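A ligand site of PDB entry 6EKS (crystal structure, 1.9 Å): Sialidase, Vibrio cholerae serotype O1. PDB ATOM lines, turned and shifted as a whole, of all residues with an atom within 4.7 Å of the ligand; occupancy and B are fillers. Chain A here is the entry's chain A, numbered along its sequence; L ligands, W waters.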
ATOM      1  N   ARG A 200      30.832 -18.518 -16.185  1.00  0.00           N
ATOM      2  CA  ARG A 200      29.776 -19.376 -15.635  1.00  0.00           C
ATOM      3  C   ARG A 200      30.248 -20.076 -14.357  1.00  0.00           C
ATOM      4  O   ARG A 200      31.433 -20.086 -14.054  1.00  0.00           O
ATOM      5  CB  ARG A 200      29.348 -20.458 -16.668  1.00  0.00           C
ATOM      6  CG  ARG A 200      28.274 -20.024 -17.712  1.00  0.00           C
ATOM      7  CD  ARG A 200      27.419 -21.235 -18.125  1.00  0.00           C
ATOM      8  NE  ARG A 200      26.512 -21.671 -17.059  1.00  0.00           N
ATOM      9  CZ  ARG A 200      25.942 -22.870 -16.992  1.00  0.00           C
ATOM     10  NH1 ARG A 200      26.172 -23.781 -17.936  1.00  0.00           N
ATOM     11  NH2 ARG A 200      25.146 -23.176 -15.986  1.00  0.00           N
ATOM     12  N   ILE A 201      29.297 -20.702 -13.655  1.00  0.00           N
ATOM     13  CA  ILE A 201      29.514 -21.686 -12.584  1.00  0.00           C
ATOM     14  C   ILE A 201      30.024 -21.040 -11.291  1.00  0.00           C
ATOM     15  O   ILE A 201      31.182 -21.240 -10.879  1.00  0.00           O
ATOM     16  CB  ILE A 201      30.505 -22.807 -13.012  1.00  0.00           C
ATOM     17  CG1 ILE A 201      30.261 -23.259 -14.460  1.00  0.00           C
ATOM     18  CG2 ILE A 201      30.327 -24.024 -12.083  1.00  0.00           C
ATOM     19  CD1 ILE A 201      28.776 -23.559 -14.760  1.00  0.00           C
ATOM     20  N   ARG A 221      35.683 -18.125 -19.135  1.00  0.00           N
ATOM     21  CA  ARG A 221      35.566 -18.988 -20.322  1.00  0.00           C
ATOM     22  C   ARG A 221      35.857 -18.210 -21.584  1.00  0.00           C
ATOM     23  O   ARG A 221      34.943 -17.632 -22.190  1.00  0.00           O
ATOM     24  CB  ARG A 221      34.170 -19.633 -20.384  1.00  0.00           C
ATOM     25  CG  ARG A 221      33.903 -20.623 -19.241  1.00  0.00           C
ATOM     26  CD  ARG A 221      32.420 -20.963 -19.107  1.00  0.00           C
ATOM     27  NE  ARG A 221      32.229 -22.216 -18.376  1.00  0.00           N
ATOM     28  CZ  ARG A 221      31.243 -23.088 -18.609  1.00  0.00           C
ATOM     29  NH1 ARG A 221      30.318 -22.816 -19.539  1.00  0.00           N
ATOM     30  NH2 ARG A 221      31.168 -24.220 -17.889  1.00  0.00           N
ATOM     31  N   ASP A 226      31.493 -25.272 -21.922  1.00  0.00           N
ATOM     32  CA  ASP A 226      32.043 -26.221 -20.966  1.00  0.00           C
ATOM     33  C   ASP A 226      33.511 -26.550 -21.223  1.00  0.00           C
ATOM     34  O   ASP A 226      34.000 -26.403 -22.344  1.00  0.00           O
ATOM     35  CB  ASP A 226      31.215 -27.501 -20.966  1.00  0.00           C
ATOM     36  CG  ASP A 226      29.909 -27.338 -20.210  1.00  0.00           C
ATOM     37  OD1 ASP A 226      29.859 -26.485 -19.300  1.00  0.00           O
ATOM     38  OD2 ASP A 226      28.943 -28.040 -20.520  1.00  0.00           O
ATOM     39  N   PRO A 227      34.216 -26.987 -20.166  1.00  0.00           N
ATOM     40  CA  PRO A 227      35.609 -27.407 -20.396  1.00  0.00           C
ATOM     41  C   PRO A 227      35.693 -28.570 -21.403  1.00  0.00           C
ATOM     42  O   PRO A 227      34.731 -29.346 -21.556  1.00  0.00           O
ATOM     43  CB  PRO A 227      36.084 -27.853 -19.011  1.00  0.00           C
ATOM     44  CG  PRO A 227      34.804 -28.205 -18.247  1.00  0.00           C
ATOM     45  CD  PRO A 227      33.800 -27.162 -18.766  1.00  0.00           C
ATOM     46  N   SER A 267      37.983 -25.855 -14.107  1.00  0.00           N
ATOM     47  CA  SER A 267      36.529 -25.805 -13.971  1.00  0.00           C
ATOM     48  C   SER A 267      36.102 -26.034 -12.532  1.00  0.00           C
ATOM     49  O   SER A 267      36.868 -26.548 -11.722  1.00  0.00           O
ATOM     50  CB  SER A 267      35.861 -26.866 -14.879  1.00  0.00           C
ATOM     51  OG  SER A 267      35.775 -28.128 -14.210  1.00  0.00           O
ATOM     52  N   ASP A 268      34.855 -25.637 -12.243  1.00  0.00           N
ATOM     53  CA  ASP A 268      34.155 -26.027 -11.012  1.00  0.00           C
ATOM     54  C   ASP A 268      34.877 -25.592  -9.735  1.00  0.00           C
ATOM     55  O   ASP A 268      35.360 -26.417  -8.950  1.00  0.00           O
ATOM     56  CB  ASP A 268      33.950 -27.556 -10.997  1.00  0.00           C
ATOM     57  CG  ASP A 268      32.966 -28.024 -12.075  1.00  0.00           C
ATOM     58  OD1 ASP A 268      31.739 -28.054 -11.801  1.00  0.00           O
ATOM     59  OD2 ASP A 268      33.407 -28.360 -13.191  1.00  0.00           O
ATOM     60  N   TRP A 287      41.588 -29.906 -16.687  1.00  0.00           N
ATOM     61  CA  TRP A 287      41.335 -30.758 -17.863  1.00  0.00           C
ATOM     62  C   TRP A 287      42.311 -30.399 -18.973  1.00  0.00           C
ATOM     63  O   TRP A 287      42.680 -29.226 -19.090  1.00  0.00           O
ATOM     64  CB  TRP A 287      39.905 -30.568 -18.398  1.00  0.00           C
ATOM     65  CG  TRP A 287      38.830 -30.579 -17.359  1.00  0.00           C
ATOM     66  CD1 TRP A 287      38.327 -29.508 -16.689  1.00  0.00           C
ATOM     67  CD2 TRP A 287      38.109 -31.724 -16.903  1.00  0.00           C
ATOM     68  NE1 TRP A 287      37.354 -29.922 -15.817  1.00  0.00           N
ATOM     69  CE2 TRP A 287      37.198 -31.282 -15.928  1.00  0.00           C
ATOM     70  CE3 TRP A 287      38.174 -33.100 -17.189  1.00  0.00           C
ATOM     71  CZ2 TRP A 287      36.331 -32.152 -15.263  1.00  0.00           C
ATOM     72  CZ3 TRP A 287      37.298 -33.958 -16.544  1.00  0.00           C
ATOM     73  CH2 TRP A 287      36.413 -33.495 -15.578  1.00  0.00           C
ATOM     74  N   GLN A 293      34.703 -33.778 -19.200  1.00  0.00           N
ATOM     75  CA  GLN A 293      33.668 -34.671 -18.707  1.00  0.00           C
ATOM     76  C   GLN A 293      32.566 -34.994 -19.728  1.00  0.00           C
ATOM     77  O   GLN A 293      32.114 -36.155 -19.829  1.00  0.00           O
ATOM     78  CB  GLN A 293      33.051 -34.049 -17.476  1.00  0.00           C
ATOM     79  CG  GLN A 293      32.711 -35.014 -16.403  1.00  0.00           C
ATOM     80  CD  GLN A 293      32.297 -34.269 -15.179  1.00  0.00           C
ATOM     81  OE1 GLN A 293      33.061 -34.150 -14.204  1.00  0.00           O
ATOM     82  NE2 GLN A 293      31.103 -33.692 -15.217  1.00  0.00           N
ATOM     83  N   ASN A 294      32.122 -33.977 -20.461  1.00  0.00           N
ATOM     84  CA  ASN A 294      31.101 -34.155 -21.504  1.00  0.00           C
ATOM     85  C   ASN A 294      31.497 -35.251 -22.504  1.00  0.00           C
ATOM     86  O   ASN A 294      32.635 -35.314 -22.962  1.00  0.00           O
ATOM     87  CB  ASN A 294      30.858 -32.847 -22.235  1.00  0.00           C
ATOM     88  CG  ASN A 294      30.169 -31.787 -21.365  1.00  0.00           C
ATOM     89  OD1 ASN A 294      29.612 -32.101 -20.299  1.00  0.00           O
ATOM     90  ND2 ASN A 294      30.192 -30.536 -21.821  1.00  0.00           N
ATOM     91  N   ASN A 521      36.370 -34.294 -10.159  1.00  0.00           N
ATOM     92  CA  ASN A 521      35.905 -32.905 -10.373  1.00  0.00           C
ATOM     93  C   ASN A 521      35.224 -32.415  -9.109  1.00  0.00           C
ATOM     94  O   ASN A 521      34.279 -33.052  -8.649  1.00  0.00           O
ATOM     95  CB  ASN A 521      34.949 -32.902 -11.582  1.00  0.00           C
ATOM     96  CG  ASN A 521      34.325 -31.522 -11.871  1.00  0.00           C
ATOM     97  OD1 ASN A 521      34.611 -30.544 -11.187  1.00  0.00           O
ATOM     98  ND2 ASN A 521      33.489 -31.456 -12.908  1.00  0.00           N
ATOM     99  N   ILE A 549      32.634 -35.050  -8.084  1.00  0.00           N
ATOM    100  CA  ILE A 549      32.061 -35.846  -9.160  1.00  0.00           C
ATOM    101  C   ILE A 549      33.161 -36.736  -9.676  1.00  0.00           C
ATOM    102  O   ILE A 549      34.221 -36.244 -10.099  1.00  0.00           O
ATOM    103  CB  ILE A 549      31.543 -34.992 -10.325  1.00  0.00           C
ATOM    104  CG1 ILE A 549      30.561 -33.924  -9.836  1.00  0.00           C
ATOM    105  CG2 ILE A 549      30.892 -35.889 -11.384  1.00  0.00           C
ATOM    106  CD1 ILE A 549      30.191 -32.923 -10.896  1.00  0.00           C
ATOM    107  N   LEU A 556      28.893 -41.193 -14.224  1.00  0.00           N
ATOM    108  CA  LEU A 556      29.179 -40.219 -13.171  1.00  0.00           C
ATOM    109  C   LEU A 556      28.561 -40.645 -11.865  1.00  0.00           C
ATOM    110  O   LEU A 556      27.481 -41.237 -11.843  1.00  0.00           O
ATOM    111  CB  LEU A 556      28.617 -38.848 -13.539  1.00  0.00           C
ATOM    112  CG  LEU A 556      29.160 -38.190 -14.788  1.00  0.00           C
ATOM    113  CD1 LEU A 556      28.302 -36.948 -15.096  1.00  0.00           C
ATOM    114  CD2 LEU A 556      30.623 -37.818 -14.604  1.00  0.00           C
ATOM    115  N   SER A 594      25.577 -36.074  -9.939  1.00  0.00           N
ATOM    116  CA  SER A 594      26.668 -35.278 -10.451  1.00  0.00           C
ATOM    117  C   SER A 594      26.884 -34.051  -9.583  1.00  0.00           C
ATOM    118  O   SER A 594      27.657 -34.078  -8.612  1.00  0.00           O
ATOM    119  CB  SER A 594      26.387 -34.867 -11.909  1.00  0.00           C
ATOM    120  OG  SER A 594      25.133 -34.185 -12.070  1.00  0.00           O
ATOM    121  N   GLU A 595      26.188 -32.975  -9.893  1.00  0.00           N
ATOM    122  CA  GLU A 595      26.450 -31.722  -9.184  1.00  0.00           C
ATOM    123  C   GLU A 595      25.762 -31.710  -7.833  1.00  0.00           C
ATOM    124  O   GLU A 595      24.545 -31.763  -7.738  1.00  0.00           O
ATOM    125  CB  GLU A 595      26.002 -30.530 -10.051  1.00  0.00           C
ATOM    126  CG  GLU A 595      26.839 -30.442 -11.323  1.00  0.00           C
ATOM    127  CD  GLU A 595      26.389 -29.347 -12.278  1.00  0.00           C
ATOM    128  OE1 GLU A 595      25.238 -28.907 -12.163  1.00  0.00           O
ATOM    129  OE2 GLU A 595      27.211 -28.948 -13.138  1.00  0.00           O
ATOM    130  N   ARG A 611      22.124 -33.243  -8.107  1.00  0.00           N
ATOM    131  CA  ARG A 611      21.532 -33.241  -9.417  1.00  0.00           C
ATOM    132  C   ARG A 611      21.660 -34.669  -9.967  1.00  0.00           C
ATOM    133  O   ARG A 611      22.719 -35.279  -9.811  1.00  0.00           O
ATOM    134  CB  ARG A 611      22.262 -32.265 -10.311  1.00  0.00           C
ATOM    135  CG  ARG A 611      21.979 -32.392 -11.788  1.00  0.00           C
ATOM    136  CD  ARG A 611      22.644 -31.238 -12.514  1.00  0.00           C
ATOM    137  NE  ARG A 611      22.468 -31.311 -13.953  1.00  0.00           N
ATOM    138  CZ  ARG A 611      22.831 -30.357 -14.795  1.00  0.00           C
ATOM    139  NH1 ARG A 611      23.368 -29.236 -14.344  1.00  0.00           N
ATOM    140  NH2 ARG A 611      22.640 -30.534 -16.114  1.00  0.00           N
ATOM    141  N   ASP A 613      21.693 -36.713 -13.388  1.00  0.00           N
ATOM    142  CA  ASP A 613      21.732 -36.487 -14.837  1.00  0.00           C
ATOM    143  C   ASP A 613      21.405 -37.720 -15.675  1.00  0.00           C
ATOM    144  O   ASP A 613      21.453 -38.862 -15.191  1.00  0.00           O
ATOM    145  CB  ASP A 613      23.094 -35.925 -15.231  1.00  0.00           C
ATOM    146  CG  ASP A 613      23.189 -34.411 -14.928  1.00  0.00           C
ATOM    147  OD1 ASP A 613      22.233 -33.666 -15.280  1.00  0.00           O
ATOM    148  OD2 ASP A 613      24.190 -33.983 -14.337  1.00  0.00           O
ATOM    149  N   PHE A 614      21.032 -37.435 -16.918  1.00  0.00           N
ATOM    150  CA  PHE A 614      20.542 -38.421 -17.889  1.00  0.00           C
ATOM    151  C   PHE A 614      19.406 -39.199 -17.273  1.00  0.00           C
ATOM    152  O   PHE A 614      18.538 -38.617 -16.642  1.00  0.00           O
ATOM    153  CB  PHE A 614      21.684 -39.319 -18.361  1.00  0.00           C
ATOM    154  CG  PHE A 614      22.910 -38.552 -18.751  1.00  0.00           C
ATOM    155  CD1 PHE A 614      22.886 -37.678 -19.838  1.00  0.00           C
ATOM    156  CD2 PHE A 614      24.074 -38.633 -17.992  1.00  0.00           C
ATOM    157  CE1 PHE A 614      24.013 -36.937 -20.195  1.00  0.00           C
ATOM    158  CE2 PHE A 614      25.196 -37.889 -18.319  1.00  0.00           C
ATOM    159  CZ  PHE A 614      25.175 -37.041 -19.434  1.00  0.00           C
ATOM    160  N   ARG A 688      15.204 -22.524 -16.601  1.00  0.00           N
ATOM    161  CA  ARG A 688      16.100 -21.930 -15.636  1.00  0.00           C
ATOM    162  C   ARG A 688      15.701 -20.446 -15.463  1.00  0.00           C
ATOM    163  O   ARG A 688      16.343 -19.535 -15.976  1.00  0.00           O
ATOM    164  CB  ARG A 688      17.549 -22.084 -16.094  1.00  0.00           C
ATOM    165  CG  ARG A 688      18.027 -23.548 -15.954  1.00  0.00           C
ATOM    166  CD  ARG A 688      19.425 -23.751 -16.498  1.00  0.00           C
ATOM    167  NE  ARG A 688      19.835 -25.151 -16.354  1.00  0.00           N
ATOM    168  CZ  ARG A 688      21.069 -25.589 -16.566  1.00  0.00           C
ATOM    169  NH1 ARG A 688      22.039 -24.755 -16.922  1.00  0.00           N
ATOM    170  NH2 ARG A 688      21.334 -26.896 -16.407  1.00  0.00           N
ATOM    171  N   TYR A 716      22.500 -21.519 -12.397  1.00  0.00           N
ATOM    172  CA  TYR A 716      23.303 -21.952 -11.226  1.00  0.00           C
ATOM    173  C   TYR A 716      23.301 -20.874 -10.155  1.00  0.00           C
ATOM    174  O   TYR A 716      23.245 -19.691 -10.448  1.00  0.00           O
ATOM    175  CB  TYR A 716      24.741 -22.267 -11.590  1.00  0.00           C
ATOM    176  CG  TYR A 716      24.938 -23.571 -12.333  1.00  0.00           C
ATOM    177  CD1 TYR A 716      23.947 -24.082 -13.167  1.00  0.00           C
ATOM    178  CD2 TYR A 716      26.137 -24.280 -12.216  1.00  0.00           C
ATOM    179  CE1 TYR A 716      24.129 -25.291 -13.875  1.00  0.00           C
ATOM    180  CE2 TYR A 716      26.337 -25.460 -12.888  1.00  0.00           C
ATOM    181  CZ  TYR A 716      25.334 -25.953 -13.726  1.00  0.00           C
ATOM    182  OH  TYR A 716      25.552 -27.120 -14.386  1.00  0.00           O
HETATM  183  C1  LIG L   1      24.745 -27.268 -17.271  1.00  0.00           C
HETATM  184  O1  LIG L   1      24.607 -26.027 -17.497  1.00  0.00           O
HETATM  185  O2  LIG L   1      23.703 -27.976 -17.252  1.00  0.00           O
HETATM  186  C2  LIG L   1      26.035 -27.819 -17.027  1.00  0.00           C
HETATM  187  C3  LIG L   1      27.190 -26.967 -17.016  1.00  0.00           C
HETATM  188  C4  LIG L   1      28.369 -27.611 -16.239  1.00  0.00           C
HETATM  189  C5  LIG L   1      28.637 -29.026 -16.816  1.00  0.00           C
HETATM  190  N1  LIG L   1      29.873 -29.596 -16.209  1.00  0.00           N
HETATM  191  C6  LIG L   1      30.982 -29.831 -16.939  1.00  0.00           C
HETATM  192  O3  LIG L   1      31.051 -29.616 -18.150  1.00  0.00           O
HETATM  193  C7  LIG L   1      32.207 -30.347 -16.153  1.00  0.00           C
HETATM  194  C8  LIG L   1      27.421 -29.846 -16.460  1.00  0.00           C
HETATM  195  C9  LIG L   1      26.179 -29.199 -16.789  1.00  0.00           C
HETATM  196  O4  LIG L   1      27.558 -31.160 -17.034  1.00  0.00           O
HETATM  197  C10 LIG L   1      26.514 -31.967 -16.457  1.00  0.00           C
HETATM  198  C11 LIG L   1      26.425 -33.299 -17.205  1.00  0.00           C
HETATM  199  C12 LIG L   1      26.718 -32.187 -14.952  1.00  0.00           C
HETATM  200  C13 LIG L   1      28.101 -32.776 -14.655  1.00  0.00           C
HETATM  201  C14 LIG L   1      25.620 -33.035 -18.486  1.00  0.00           C
HETATM  202  N2  LIG L   1      29.585 -26.799 -16.358  1.00  0.00           N
HETATM  203  O   HOH W   1      29.860 -33.078 -17.781  1.00  0.00           O
HETATM  204  O   HOH W   2      29.365 -27.059 -12.950  1.00  0.00           O
HETATM  205  O   HOH W   3      32.149 -26.843 -15.377  1.00  0.00           O
HETATM  206  O   HOH W   4      32.938 -31.119 -19.858  1.00  0.00           O
HETATM  207  O   HOH W   5      21.496 -27.607 -19.326  1.00  0.00           O
HETATM  208  O   HOH W   6      30.107 -29.616 -13.460  1.00  0.00           O
HETATM  209  O   HOH W   7      25.071 -26.507 -20.589  1.00  0.00           O
HETATM  210  O   HOH W   8      27.013 -30.423 -19.830  1.00  0.00           O
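An oxygen (O2) of the ligand is in salt-bridge range of the guanidinium group (NH2) of Arg 688 (2.7 Å).
NH1 of Arg 200 is in salt-bridge range of O1 of the ligand, at 2.8 Å.
O1 of the ligand sits close to OH of Tyr 716 (3.4 Å).
The side-chain carboxylate (OD1) of Asp 226 lies within salt-bridge range of a nitrogen (N2) of the ligand (3.0 Å).
O2 of the ligand is in salt-bridge range of NH2 of Arg 611 (3.0 Å).
A nitrogen (N2) of the ligand lies close to the guanidinium group of Arg 221, 3.4 Å away.
The guanidinium group (NH1) of Arg 611 is in hydrogen-bond range of the side-chain hydroxyl (OH) of Tyr 716 (3.0 Å).
The side-chain carboxylate (OE2) of Glu 595 lies within hydrogen-bond range of the side-chain hydroxyl (OH) of Tyr 716 (2.8 Å).
The side-chain carboxylate of Asp 226 is in hydrogen-bond range of the side-chain amide nitrogen of Asn 294.
NE of Arg 611 lies within salt-bridge range of OD1 of Asp 613 (2.7 Å).
NH1 of Arg 611 is in salt-bridge range of OE1 of Glu 595 (2.9 Å).
The backbone carbonyl oxygen of Arg 611 is in hydrogen-bond range of the backbone NH of Ser 594.
OG of Ser 594 sits at hydrogen-bond distance from OD2 of Asp 613 (2.5 Å).
The backbone carbonyl oxygen (O) of Asn 521 sits at hydrogen-bond distance from the backbone NH (N) of Ile 549, 2.6 Å away.
Residues that only touch the ligand: Asp 613 (3.2 Å), Gln 293 (3.2 Å), Glu 595 (3.4 Å), Asn 294 (3.6 Å), Asn 521 (3.7 Å), Ile 201 (3.7 Å), Pro 227 (3.7 Å), Asp 268 (3.8 Å) and Ser 594 (3.8 Å).
Hydrophobic or aromatic side chains within 4 Å of the ligand: Ile 201, Pro 227 and Tyr 716.
Of the 20 residues printed, 15 come within 4 Å of the ligand.
The nearest printed residue that does not touch the ligand is Phe 614 (4.1 Å).
Water W3 lies within hydrogen-bond range of a nitrogen (N2) of the ligand (2.7 Å) and the side-chain carboxylate (OD2) of Asp 268 (2.9 Å).
Water W6 lies within hydrogen-bond range of a nitrogen (N1) of the ligand (2.8 Å), the side-chain carboxylate (OD1) of Asp 268 (2.8 Å) and the side-chain carboxylate (OE2) of Glu 595 (3.0 Å).
Water W4 lies within hydrogen-bond range of an oxygen (O3) of the ligand (3.0 Å), the backbone NH of Asn 294 (3.0 Å), the backbone carbonyl oxygen of Pro 227 (3.0 Å) and the backbone NH of Gln 293 (3.3 Å).
Water W5 lies within hydrogen-bond range of the guanidinium group (NH2) of Arg 688 (3.0 Å) and an oxygen (O2) of the ligand (3.1 Å).
Water W1 lies within hydrogen-bond range of the side-chain amide oxygen (OD1) of Asn 294 (2.7 Å), the side-chain amide nitrogen (NE2) of Gln 293 (2.9 Å) and an oxygen (O4) of the ligand (3.1 Å).
Water W2 lies within hydrogen-bond range of the side-chain carboxylate (OD1) of Asp 268 (2.8 Å), the side-chain carboxylate (OE2) of Glu 595 (2.9 Å) and a nitrogen (N2) of the ligand (3.4 Å).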
